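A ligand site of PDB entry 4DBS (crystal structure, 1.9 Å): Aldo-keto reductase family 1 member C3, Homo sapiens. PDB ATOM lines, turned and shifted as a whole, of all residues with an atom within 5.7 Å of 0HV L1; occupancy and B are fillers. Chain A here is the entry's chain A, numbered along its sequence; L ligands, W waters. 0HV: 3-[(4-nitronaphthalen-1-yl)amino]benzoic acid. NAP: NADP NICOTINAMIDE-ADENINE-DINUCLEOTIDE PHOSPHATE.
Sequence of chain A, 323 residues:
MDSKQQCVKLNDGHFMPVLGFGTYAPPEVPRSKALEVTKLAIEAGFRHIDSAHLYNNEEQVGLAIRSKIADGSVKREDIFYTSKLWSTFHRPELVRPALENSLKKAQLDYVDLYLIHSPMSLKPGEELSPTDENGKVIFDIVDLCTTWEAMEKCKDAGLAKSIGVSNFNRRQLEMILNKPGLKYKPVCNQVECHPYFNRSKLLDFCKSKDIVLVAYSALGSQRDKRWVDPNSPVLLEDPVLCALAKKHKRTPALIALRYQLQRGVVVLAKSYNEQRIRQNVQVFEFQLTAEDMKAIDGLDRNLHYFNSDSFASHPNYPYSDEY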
ATOM      1  N   TYR A  24     -34.880  -6.462  -6.251  1.00  0.00           N
ATOM      2  CA  TYR A  24     -34.865  -5.115  -5.700  1.00  0.00           C
ATOM      3  C   TYR A  24     -36.242  -4.492  -5.568  1.00  0.00           C
ATOM      4  O   TYR A  24     -37.022  -4.469  -6.516  1.00  0.00           O
ATOM      5  CB  TYR A  24     -33.961  -4.147  -6.476  1.00  0.00           C
ATOM      6  CG  TYR A  24     -33.918  -2.806  -5.788  1.00  0.00           C
ATOM      7  CD1 TYR A  24     -33.188  -2.645  -4.615  1.00  0.00           C
ATOM      8  CD2 TYR A  24     -34.630  -1.718  -6.276  1.00  0.00           C
ATOM      9  CE1 TYR A  24     -33.161  -1.440  -3.949  1.00  0.00           C
ATOM     10  CE2 TYR A  24     -34.605  -0.497  -5.624  1.00  0.00           C
ATOM     11  CZ  TYR A  24     -33.859  -0.365  -4.453  1.00  0.00           C
ATOM     12  OH  TYR A  24     -33.821   0.836  -3.799  1.00  0.00           O
ATOM     13  N   LEU A  54     -26.487  -4.435  -1.883  1.00  0.00           N
ATOM     14  CA  LEU A  54     -27.183  -3.153  -2.026  1.00  0.00           C
ATOM     15  C   LEU A  54     -28.674  -3.221  -1.700  1.00  0.00           C
ATOM     16  O   LEU A  54     -29.261  -2.248  -1.216  1.00  0.00           O
ATOM     17  CB  LEU A  54     -27.031  -2.641  -3.445  1.00  0.00           C
ATOM     18  CG  LEU A  54     -27.732  -1.312  -3.709  1.00  0.00           C
ATOM     19  CD1 LEU A  54     -27.061  -0.204  -2.903  1.00  0.00           C
ATOM     20  CD2 LEU A  54     -27.716  -0.995  -5.198  1.00  0.00           C
ATOM     21  N   TYR A  55     -29.293  -4.365  -1.984  1.00  0.00           N
ATOM     22  CA  TYR A  55     -30.752  -4.444  -1.996  1.00  0.00           C
ATOM     23  C   TYR A  55     -31.343  -4.552  -0.594  1.00  0.00           C
ATOM     24  O   TYR A  55     -32.543  -4.462  -0.411  1.00  0.00           O
ATOM     25  CB  TYR A  55     -31.239  -5.606  -2.852  1.00  0.00           C
ATOM     26  CG  TYR A  55     -30.791  -5.550  -4.302  1.00  0.00           C
ATOM     27  CD1 TYR A  55     -31.011  -6.614  -5.163  1.00  0.00           C
ATOM     28  CD2 TYR A  55     -30.166  -4.426  -4.810  1.00  0.00           C
ATOM     29  CE1 TYR A  55     -30.615  -6.569  -6.474  1.00  0.00           C
ATOM     30  CE2 TYR A  55     -29.763  -4.363  -6.136  1.00  0.00           C
ATOM     31  CZ  TYR A  55     -29.983  -5.433  -6.957  1.00  0.00           C
ATOM     32  OH  TYR A  55     -29.577  -5.390  -8.259  1.00  0.00           O
ATOM     33  N   LYS A  84     -23.988  -9.554  -5.328  1.00  0.00           N
ATOM     34  CA  LYS A  84     -23.128  -8.582  -5.971  1.00  0.00           C
ATOM     35  C   LYS A  84     -22.308  -7.833  -4.936  1.00  0.00           C
ATOM     36  O   LYS A  84     -22.809  -7.481  -3.873  1.00  0.00           O
ATOM     37  CB  LYS A  84     -23.946  -7.584  -6.802  1.00  0.00           C
ATOM     38  CG  LYS A  84     -24.995  -8.210  -7.735  1.00  0.00           C
ATOM     39  CD  LYS A  84     -25.558  -7.137  -8.687  1.00  0.00           C
ATOM     40  CE  LYS A  84     -26.744  -7.646  -9.515  1.00  0.00           C
ATOM     41  NZ  LYS A  84     -27.968  -7.812  -8.679  1.00  0.00           N
ATOM     42  N   HIS A 117     -20.862  -5.116  -8.660  1.00  0.00           N
ATOM     43  CA  HIS A 117     -22.135  -4.438  -8.942  1.00  0.00           C
ATOM     44  C   HIS A 117     -21.951  -3.275  -9.922  1.00  0.00           C
ATOM     45  O   HIS A 117     -22.842  -3.000 -10.733  1.00  0.00           O
ATOM     46  CB  HIS A 117     -22.757  -3.908  -7.642  1.00  0.00           C
ATOM     47  CG  HIS A 117     -24.253  -3.721  -7.709  1.00  0.00           C
ATOM     48  ND1 HIS A 117     -25.089  -4.094  -6.691  1.00  0.00           N
ATOM     49  CD2 HIS A 117     -25.043  -3.190  -8.671  1.00  0.00           C
ATOM     50  CE1 HIS A 117     -26.340  -3.812  -7.011  1.00  0.00           C
ATOM     51  NE2 HIS A 117     -26.344  -3.263  -8.215  1.00  0.00           N
ATOM     52  N   MET A 120     -18.032   1.854 -10.564  1.00  0.00           N
ATOM     53  CA  MET A 120     -17.909   3.155  -9.928  1.00  0.00           C
ATOM     54  C   MET A 120     -17.610   3.059  -8.429  1.00  0.00           C
ATOM     55  O   MET A 120     -18.501   3.185  -7.589  1.00  0.00           O
ATOM     56  CB  MET A 120     -19.153   4.006 -10.217  1.00  0.00           C
ATOM     57  CG  MET A 120     -19.239   4.435 -11.680  1.00  0.00           C
ATOM     58  SD  MET A 120     -20.785   5.281 -12.045  1.00  0.00           S
ATOM     59  CE  MET A 120     -21.916   3.898 -12.089  1.00  0.00           C
ATOM     60  N   ASN A 167     -22.702  -3.470 -15.108  1.00  0.00           N
ATOM     61  CA  ASN A 167     -22.591  -2.057 -15.492  1.00  0.00           C
ATOM     62  C   ASN A 167     -21.222  -1.663 -16.062  1.00  0.00           C
ATOM     63  O   ASN A 167     -20.854  -0.494 -16.069  1.00  0.00           O
ATOM     64  CB  ASN A 167     -23.003  -1.143 -14.341  1.00  0.00           C
ATOM     65  CG  ASN A 167     -24.456  -1.383 -13.922  1.00  0.00           C
ATOM     66  OD1 ASN A 167     -25.349  -1.422 -14.770  1.00  0.00           O
ATOM     67  ND2 ASN A 167     -24.686  -1.555 -12.624  1.00  0.00           N
ATOM     68  N   GLN A 190     -23.872  -7.909 -16.473  1.00  0.00           N
ATOM     69  CA  GLN A 190     -25.259  -7.532 -16.223  1.00  0.00           C
ATOM     70  C   GLN A 190     -25.425  -6.027 -16.398  1.00  0.00           C
ATOM     71  O   GLN A 190     -24.848  -5.232 -15.647  1.00  0.00           O
ATOM     72  CB  GLN A 190     -25.702  -7.951 -14.820  1.00  0.00           C
ATOM     73  CG  GLN A 190     -27.169  -7.585 -14.528  1.00  0.00           C
ATOM     74  CD  GLN A 190     -27.621  -7.954 -13.116  1.00  0.00           C
ATOM     75  OE1 GLN A 190     -28.208  -7.125 -12.410  1.00  0.00           O
ATOM     76  NE2 GLN A 190     -27.357  -9.197 -12.703  1.00  0.00           N
ATOM     77  N   TYR A 216     -31.074  -6.123 -17.336  1.00  0.00           N
ATOM     78  CA  TYR A 216     -31.970  -5.607 -16.299  1.00  0.00           C
ATOM     79  C   TYR A 216     -32.755  -4.391 -16.787  1.00  0.00           C
ATOM     80  O   TYR A 216     -32.409  -3.782 -17.810  1.00  0.00           O
ATOM     81  CB  TYR A 216     -31.220  -5.294 -15.003  1.00  0.00           C
ATOM     82  CG  TYR A 216     -30.323  -4.071 -15.001  1.00  0.00           C
ATOM     83  CD1 TYR A 216     -28.951  -4.198 -14.872  1.00  0.00           C
ATOM     84  CD2 TYR A 216     -30.858  -2.783 -15.084  1.00  0.00           C
ATOM     85  CE1 TYR A 216     -28.117  -3.081 -14.855  1.00  0.00           C
ATOM     86  CE2 TYR A 216     -30.044  -1.670 -15.067  1.00  0.00           C
ATOM     87  CZ  TYR A 216     -28.677  -1.822 -14.959  1.00  0.00           C
ATOM     88  OH  TYR A 216     -27.862  -0.713 -14.933  1.00  0.00           O
ATOM     89  N   TRP A 227     -33.724   8.247  -9.607  1.00  0.00           N
ATOM     90  CA  TRP A 227     -32.821   8.105 -10.756  1.00  0.00           C
ATOM     91  C   TRP A 227     -33.483   8.217 -12.114  1.00  0.00           C
ATOM     92  O   TRP A 227     -32.802   8.432 -13.112  1.00  0.00           O
ATOM     93  CB  TRP A 227     -32.083   6.769 -10.700  1.00  0.00           C
ATOM     94  CG  TRP A 227     -31.416   6.529  -9.403  1.00  0.00           C
ATOM     95  CD1 TRP A 227     -30.257   7.077  -8.957  1.00  0.00           C
ATOM     96  CD2 TRP A 227     -31.880   5.669  -8.356  1.00  0.00           C
ATOM     97  NE1 TRP A 227     -29.968   6.625  -7.695  1.00  0.00           N
ATOM     98  CE2 TRP A 227     -30.950   5.755  -7.308  1.00  0.00           C
ATOM     99  CE3 TRP A 227     -32.983   4.829  -8.210  1.00  0.00           C
ATOM    100  CZ2 TRP A 227     -31.089   5.043  -6.119  1.00  0.00           C
ATOM    101  CZ3 TRP A 227     -33.133   4.122  -7.041  1.00  0.00           C
ATOM    102  CH2 TRP A 227     -32.185   4.228  -6.007  1.00  0.00           C
ATOM    103  N   PHE A 306     -31.820   4.905 -15.877  1.00  0.00           N
ATOM    104  CA  PHE A 306     -31.073   5.369 -14.714  1.00  0.00           C
ATOM    105  C   PHE A 306     -30.183   6.570 -15.043  1.00  0.00           C
ATOM    106  O   PHE A 306     -29.341   6.500 -15.935  1.00  0.00           O
ATOM    107  CB  PHE A 306     -30.213   4.233 -14.144  1.00  0.00           C
ATOM    108  CG  PHE A 306     -31.019   3.181 -13.438  1.00  0.00           C
ATOM    109  CD1 PHE A 306     -31.547   2.108 -14.128  1.00  0.00           C
ATOM    110  CD2 PHE A 306     -31.260   3.287 -12.074  1.00  0.00           C
ATOM    111  CE1 PHE A 306     -32.308   1.151 -13.473  1.00  0.00           C
ATOM    112  CE2 PHE A 306     -32.011   2.327 -11.409  1.00  0.00           C
ATOM    113  CZ  PHE A 306     -32.528   1.251 -12.112  1.00  0.00           C
ATOM    114  N   ASN A 307     -30.372   7.668 -14.323  1.00  0.00           N
ATOM    115  CA  ASN A 307     -29.511   8.838 -14.479  1.00  0.00           C
ATOM    116  C   ASN A 307     -28.983   9.360 -13.156  1.00  0.00           C
ATOM    117  O   ASN A 307     -29.631   9.233 -12.114  1.00  0.00           O
ATOM    118  CB  ASN A 307     -30.244   9.969 -15.219  1.00  0.00           C
ATOM    119  CG  ASN A 307     -30.136   9.840 -16.726  1.00  0.00           C
ATOM    120  OD1 ASN A 307     -29.114  10.184 -17.311  1.00  0.00           O
ATOM    121  ND2 ASN A 307     -31.187   9.341 -17.351  1.00  0.00           N
ATOM    122  N   SER A 308     -27.797   9.943 -13.192  1.00  0.00           N
ATOM    123  CA  SER A 308     -27.207  10.541 -12.003  1.00  0.00           C
ATOM    124  C   SER A 308     -26.221  11.620 -12.416  1.00  0.00           C
ATOM    125  O   SER A 308     -25.155  11.319 -12.956  1.00  0.00           O
ATOM    126  CB  SER A 308     -26.503   9.489 -11.145  1.00  0.00           C
ATOM    127  OG  SER A 308     -25.750  10.111 -10.126  1.00  0.00           O
ATOM    128  N   PHE A 311     -22.782  11.020 -10.528  1.00  0.00           N
ATOM    129  CA  PHE A 311     -21.964   9.886 -10.966  1.00  0.00           C
ATOM    130  C   PHE A 311     -21.583   9.979 -12.430  1.00  0.00           C
ATOM    131  O   PHE A 311     -20.707   9.259 -12.891  1.00  0.00           O
ATOM    132  CB  PHE A 311     -22.680   8.567 -10.670  1.00  0.00           C
ATOM    133  CG  PHE A 311     -22.563   8.146  -9.239  1.00  0.00           C
ATOM    134  CD1 PHE A 311     -23.314   8.765  -8.253  1.00  0.00           C
ATOM    135  CD2 PHE A 311     -21.680   7.137  -8.867  1.00  0.00           C
ATOM    136  CE1 PHE A 311     -23.212   8.386  -6.933  1.00  0.00           C
ATOM    137  CE2 PHE A 311     -21.568   6.759  -7.546  1.00  0.00           C
ATOM    138  CZ  PHE A 311     -22.327   7.372  -6.574  1.00  0.00           C
ATOM    139  N   TYR A 317     -17.692   6.037 -14.761  1.00  0.00           N
ATOM    140  CA  TYR A 317     -19.061   6.102 -15.279  1.00  0.00           C
ATOM    141  C   TYR A 317     -19.117   5.328 -16.593  1.00  0.00           C
ATOM    142  O   TYR A 317     -18.333   5.582 -17.505  1.00  0.00           O
ATOM    143  CB  TYR A 317     -19.452   7.565 -15.483  1.00  0.00           C
ATOM    144  CG  TYR A 317     -20.862   7.798 -15.976  1.00  0.00           C
ATOM    145  CD1 TYR A 317     -21.955   7.425 -15.216  1.00  0.00           C
ATOM    146  CD2 TYR A 317     -21.088   8.452 -17.193  1.00  0.00           C
ATOM    147  CE1 TYR A 317     -23.246   7.661 -15.660  1.00  0.00           C
ATOM    148  CE2 TYR A 317     -22.369   8.690 -17.637  1.00  0.00           C
ATOM    149  CZ  TYR A 317     -23.448   8.293 -16.866  1.00  0.00           C
ATOM    150  OH  TYR A 317     -24.728   8.531 -17.309  1.00  0.00           O
ATOM    151  N   PRO A 318     -20.035   4.348 -16.692  1.00  0.00           N
ATOM    152  CA  PRO A 318     -20.060   3.438 -17.846  1.00  0.00           C
ATOM    153  C   PRO A 318     -20.552   4.060 -19.139  1.00  0.00           C
ATOM    154  O   PRO A 318     -20.205   3.548 -20.205  1.00  0.00           O
ATOM    155  CB  PRO A 318     -21.045   2.349 -17.405  1.00  0.00           C
ATOM    156  CG  PRO A 318     -21.848   2.963 -16.322  1.00  0.00           C
ATOM    157  CD  PRO A 318     -20.929   3.893 -15.608  1.00  0.00           C
ATOM    158  N   TYR A 319     -21.355   5.114 -19.067  1.00  0.00           N
ATOM    159  CA  TYR A 319     -22.004   5.635 -20.265  1.00  0.00           C
ATOM    160  C   TYR A 319     -21.232   6.800 -20.860  1.00  0.00           C
ATOM    161  O   TYR A 319     -21.811   7.727 -21.428  1.00  0.00           O
ATOM    162  CB  TYR A 319     -23.448   6.034 -19.960  1.00  0.00           C
ATOM    163  CG  TYR A 319     -24.273   4.887 -19.409  1.00  0.00           C
ATOM    164  CD1 TYR A 319     -24.317   3.663 -20.061  1.00  0.00           C
ATOM    165  CD2 TYR A 319     -25.024   5.030 -18.245  1.00  0.00           C
ATOM    166  CE1 TYR A 319     -25.074   2.596 -19.567  1.00  0.00           C
ATOM    167  CE2 TYR A 319     -25.772   3.970 -17.738  1.00  0.00           C
ATOM    168  CZ  TYR A 319     -25.799   2.766 -18.405  1.00  0.00           C
ATOM    169  OH  TYR A 319     -26.559   1.718 -17.903  1.00  0.00           O
HETATM  170  C01 0HV L   1     -31.303  -0.305  -7.818  1.00  0.00           C
HETATM  171  C02 0HV L   1     -31.384   1.036  -7.760  1.00  0.00           C
HETATM  172  C03 0HV L   1     -30.528   1.810  -8.459  1.00  0.00           C
HETATM  173  C04 0HV L   1     -29.538   1.293  -9.232  1.00  0.00           C
HETATM  174  C05 0HV L   1     -29.485  -0.063  -9.263  1.00  0.00           C
HETATM  175  C06 0HV L   1     -30.336  -0.865  -8.575  1.00  0.00           C
HETATM  176  N07 0HV L   1     -28.846   2.176  -9.871  1.00  0.00           N
HETATM  177  C08 0HV L   1     -28.070   2.319 -10.891  1.00  0.00           C
HETATM  178  C09 0HV L   1     -27.438   1.282 -11.466  1.00  0.00           C
HETATM  179  C10 0HV L   1     -26.589   1.414 -12.504  1.00  0.00           C
HETATM  180  C11 0HV L   1     -26.311   2.612 -13.066  1.00  0.00           C
HETATM  181  C12 0HV L   1     -26.939   3.690 -12.507  1.00  0.00           C
HETATM  182  C13 0HV L   1     -27.798   3.546 -11.441  1.00  0.00           C
HETATM  183  C14 0HV L   1     -26.733   4.933 -12.994  1.00  0.00           C
HETATM  184  C15 0HV L   1     -27.313   6.033 -12.494  1.00  0.00           C
HETATM  185  C16 0HV L   1     -28.151   5.893 -11.459  1.00  0.00           C
HETATM  186  C17 0HV L   1     -28.372   4.676 -10.961  1.00  0.00           C
HETATM  187  C18 0HV L   1     -30.278  -2.233  -8.685  1.00  0.00           C
HETATM  188  O19 0HV L   1     -31.308  -2.882  -8.736  1.00  0.00           O
HETATM  189  O20 0HV L   1     -29.115  -2.916  -8.799  1.00  0.00           O
HETATM  190  N21 0HV L   1     -25.460   2.607 -14.007  1.00  0.00           N
HETATM  191  O22 0HV L   1     -24.561   3.524 -14.276  1.00  0.00           O
HETATM  192  O23 0HV L   1     -25.301   1.645 -14.888  1.00  0.00           O
HETATM  193  PA  NAP L   2     -37.980  -4.416 -14.188  1.00  0.00           P
HETATM  194  O1A NAP L   2     -37.626  -3.601 -15.366  1.00  0.00           O
HETATM  195  O2A NAP L   2     -37.592  -5.960 -14.436  1.00  0.00           O
HETATM  196  O5B NAP L   2     -39.563  -4.422 -13.897  1.00  0.00           O
HETATM  197  C5B NAP L   2     -40.033  -3.079 -13.757  1.00  0.00           C
HETATM  198  C4B NAP L   2     -41.499  -3.142 -13.322  1.00  0.00           C
HETATM  199  O4B NAP L   2     -42.199  -4.024 -14.188  1.00  0.00           O
HETATM  200  C3B NAP L   2     -41.619  -3.769 -11.929  1.00  0.00           C
HETATM  201  O3B NAP L   2     -41.597  -2.755 -10.928  1.00  0.00           O
HETATM  202  C2B NAP L   2     -42.967  -4.566 -11.981  1.00  0.00           C
HETATM  203  O2B NAP L   2     -43.995  -3.958 -11.182  1.00  0.00           O
HETATM  204  C1B NAP L   2     -43.367  -4.475 -13.488  1.00  0.00           C
HETATM  205  N9A NAP L   2     -43.770  -5.753 -14.071  1.00  0.00           N
HETATM  206  C8A NAP L   2     -43.169  -6.966 -13.896  1.00  0.00           C
HETATM  207  N7A NAP L   2     -43.800  -7.863 -14.610  1.00  0.00           N
HETATM  208  C5A NAP L   2     -44.813  -7.270 -15.291  1.00  0.00           C
HETATM  209  C6A NAP L   2     -45.795  -7.708 -16.196  1.00  0.00           C
HETATM  210  N6A NAP L   2     -45.867  -9.046 -16.580  1.00  0.00           N
HETATM  211  N1A NAP L   2     -46.654  -6.814 -16.679  1.00  0.00           N
HETATM  212  C2A NAP L   2     -46.600  -5.542 -16.331  1.00  0.00           C
HETATM  213  N3A NAP L   2     -45.700  -5.084 -15.489  1.00  0.00           N
HETATM  214  C4A NAP L   2     -44.803  -5.915 -14.951  1.00  0.00           C
HETATM  215  O3  NAP L   2     -37.358  -3.858 -12.800  1.00  0.00           O
HETATM  216  PN  NAP L   2     -35.770  -3.626 -12.561  1.00  0.00           P
HETATM  217  O1N NAP L   2     -35.685  -3.557 -11.032  1.00  0.00           O
HETATM  218  O2N NAP L   2     -35.271  -2.261 -13.077  1.00  0.00           O
HETATM  219  O5D NAP L   2     -34.813  -4.773 -13.172  1.00  0.00           O
HETATM  220  C5D NAP L   2     -35.162  -6.028 -12.587  1.00  0.00           C
HETATM  221  C4D NAP L   2     -34.046  -6.558 -11.659  1.00  0.00           C
HETATM  222  O4D NAP L   2     -32.746  -6.392 -12.294  1.00  0.00           O
HETATM  223  C3D NAP L   2     -33.941  -5.771 -10.354  1.00  0.00           C
HETATM  224  O3D NAP L   2     -34.894  -6.220  -9.393  1.00  0.00           O
HETATM  225  C2D NAP L   2     -32.505  -6.134  -9.934  1.00  0.00           C
HETATM  226  O2D NAP L   2     -32.517  -7.449  -9.365  1.00  0.00           O
HETATM  227  C1D NAP L   2     -31.750  -6.105 -11.277  1.00  0.00           C
HETATM  228  N1N NAP L   2     -31.138  -4.783 -11.525  1.00  0.00           N
HETATM  229  C2N NAP L   2     -29.818  -4.666 -11.481  1.00  0.00           C
HETATM  230  C3N NAP L   2     -29.212  -3.435 -11.667  1.00  0.00           C
HETATM  231  C7N NAP L   2     -27.739  -3.323 -11.621  1.00  0.00           C
HETATM  232  O7N NAP L   2     -27.230  -2.232 -11.449  1.00  0.00           O
HETATM  233  N7N NAP L   2     -26.977  -4.426 -11.754  1.00  0.00           N
HETATM  234  C4N NAP L   2     -30.010  -2.303 -11.897  1.00  0.00           C
HETATM  235  C5N NAP L   2     -31.381  -2.477 -11.929  1.00  0.00           C
HETATM  236  C6N NAP L   2     -31.910  -3.740 -11.737  1.00  0.00           C
HETATM  237  P2B NAP L   2     -44.631  -4.996 -10.101  1.00  0.00           P
HETATM  238  O1X NAP L   2     -43.649  -5.310  -9.040  1.00  0.00           O
HETATM  239  O2X NAP L   2     -45.895  -4.239  -9.459  1.00  0.00           O
HETATM  240  O3X NAP L   2     -45.129  -6.348 -10.816  1.00  0.00           O
HETATM  241  C01 0HV L   3     -29.766   2.483  -2.795  1.00  0.00           C
HETATM  242  C02 0HV L   3     -29.938   2.058  -4.052  1.00  0.00           C
HETATM  243  C03 0HV L   3     -29.161   2.531  -5.050  1.00  0.00           C
HETATM  244  C04 0HV L   3     -28.193   3.443  -4.839  1.00  0.00           C
HETATM  245  C05 0HV L   3     -28.048   3.839  -3.549  1.00  0.00           C
HETATM  246  C06 0HV L   3     -28.812   3.402  -2.527  1.00  0.00           C
HETATM  247  N07 0HV L   3     -27.530   3.768  -5.901  1.00  0.00           N
HETATM  248  C08 0HV L   3     -26.859   3.245  -6.867  1.00  0.00           C
HETATM  249  C09 0HV L   3     -26.667   1.917  -6.957  1.00  0.00           C
HETATM  250  C10 0HV L   3     -25.945   1.347  -7.944  1.00  0.00           C
HETATM  251  C11 0HV L   3     -25.335   2.062  -8.914  1.00  0.00           C
HETATM  252  C12 0HV L   3     -25.500   3.412  -8.838  1.00  0.00           C
HETATM  253  C13 0HV L   3     -26.245   3.997  -7.844  1.00  0.00           C
HETATM  254  C14 0HV L   3     -24.929   4.224  -9.768  1.00  0.00           C
HETATM  255  C15 0HV L   3     -25.048   5.558  -9.765  1.00  0.00           C
HETATM  256  C16 0HV L   3     -25.768   6.123  -8.791  1.00  0.00           C
HETATM  257  C17 0HV L   3     -26.355   5.343  -7.869  1.00  0.00           C
HETATM  258  C18 0HV L   3     -28.609   3.818  -1.232  1.00  0.00           C
HETATM  259  O19 0HV L   3     -27.671   4.540  -0.944  1.00  0.00           O
HETATM  260  O20 0HV L   3     -29.424   3.436  -0.208  1.00  0.00           O
HETATM  261  N21 0HV L   3     -24.650   1.382  -9.727  1.00  0.00           N
HETATM  262  O22 0HV L   3     -23.753   1.788 -10.606  1.00  0.00           O
HETATM  263  O23 0HV L   3     -24.704   0.063  -9.793  1.00  0.00           O
HETATM  264  O   HOH W   1     -33.896  -1.930  -9.564  1.00  0.00           O
HETATM  265  O   HOH W   2     -28.302   2.007 -16.027  1.00  0.00           O
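The side-chain amide nitrogen (ND2) of Asn 167 sits at hydrogen-bond distance from an oxygen (O23) of 0HV L3 (3.3 Å).
The side-chain hydroxyl (OH) of Tyr 216 lies close to an oxygen (O23) of 0HV L1 (3.5 Å).
The side-chain hydroxyl of Tyr 55 sits at hydrogen-bond distance from an oxygen (O20) of 0HV L1 (2.6 Å).
OE1 of Gln 190 lies within hydrogen-bond range of N7N of NAP L2 (3.0 Å).
The side-chain hydroxyl (OH) of Tyr 319 lies within hydrogen-bond range of an oxygen (O23) of 0HV L1 (3.3 Å).
An oxygen (O3D) of NAP L2 is in hydrogen-bond range of the backbone NH of Tyr 24.
ND2 of Asn 167 lies within hydrogen-bond range of O7N of NAP L2 (2.9 Å).
The side-chain amide oxygen (OD1) of Asn 167 sits close to an oxygen (O23) of 0HV L1 (3.1 Å).
A ring nitrogen (NE2) of His 117 lies within hydrogen-bond range of an oxygen (O20) of 0HV L1 (2.9 Å).
OH of Tyr 55 lies within hydrogen-bond range of NZ of Lys 84, at 2.9 Å.
O of His 117 lies within hydrogen-bond range of ND2 of Asn 167 (3.0 Å).
OH of Tyr 216 lies within hydrogen-bond range of OD1 of Asn 167 (2.6 Å).
N of Phe 311 is in hydrogen-bond range of OG of Ser 308, at 3.1 Å.
The backbone carbonyl oxygen (O) of Trp 227 sits at hydrogen-bond distance from the backbone NH (N) of Asn 307 (2.8 Å).
The backbone carbonyl oxygen (O) of Gln 190 sits at hydrogen-bond distance from the backbone NH (N) of Asn 167 (2.8 Å).
Tyr 24 touches 0HV L1 (CB to O19, 3.7 Å).
Met 120 touches 0HV L1 (CE to O22, 3.5 Å).
Trp 227 touches 0HV L1 (CD1 to C16, 3.5 Å).
Phe 306 touches 0HV L1.
O of Asn 307 touches C16 of 0HV L1 (3.7 Å).
CB of Ser 308 touches C15 of 0HV L1, at 3.8 Å.
Pro 318 touches 0HV L1.
Within 4 Å of 0HV L1: Tyr 24, Tyr 55, His 117, Met 120, Asn 167, Tyr 216, Trp 227, Phe 306, Asn 307, Ser 308, Pro 318 and Tyr 319.
Water W1 lies within hydrogen-bond range of an oxygen (O1N) of NAP L2 (2.8 Å) and an oxygen (O19) of 0HV L1 (2.9 Å).
Water W2 lies within hydrogen-bond range of the side-chain hydroxyl of Tyr 319 (2.6 Å), the side-chain hydroxyl of Tyr 216 (3.0 Å) and an oxygen (O23) of 0HV L1 (3.2 Å).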
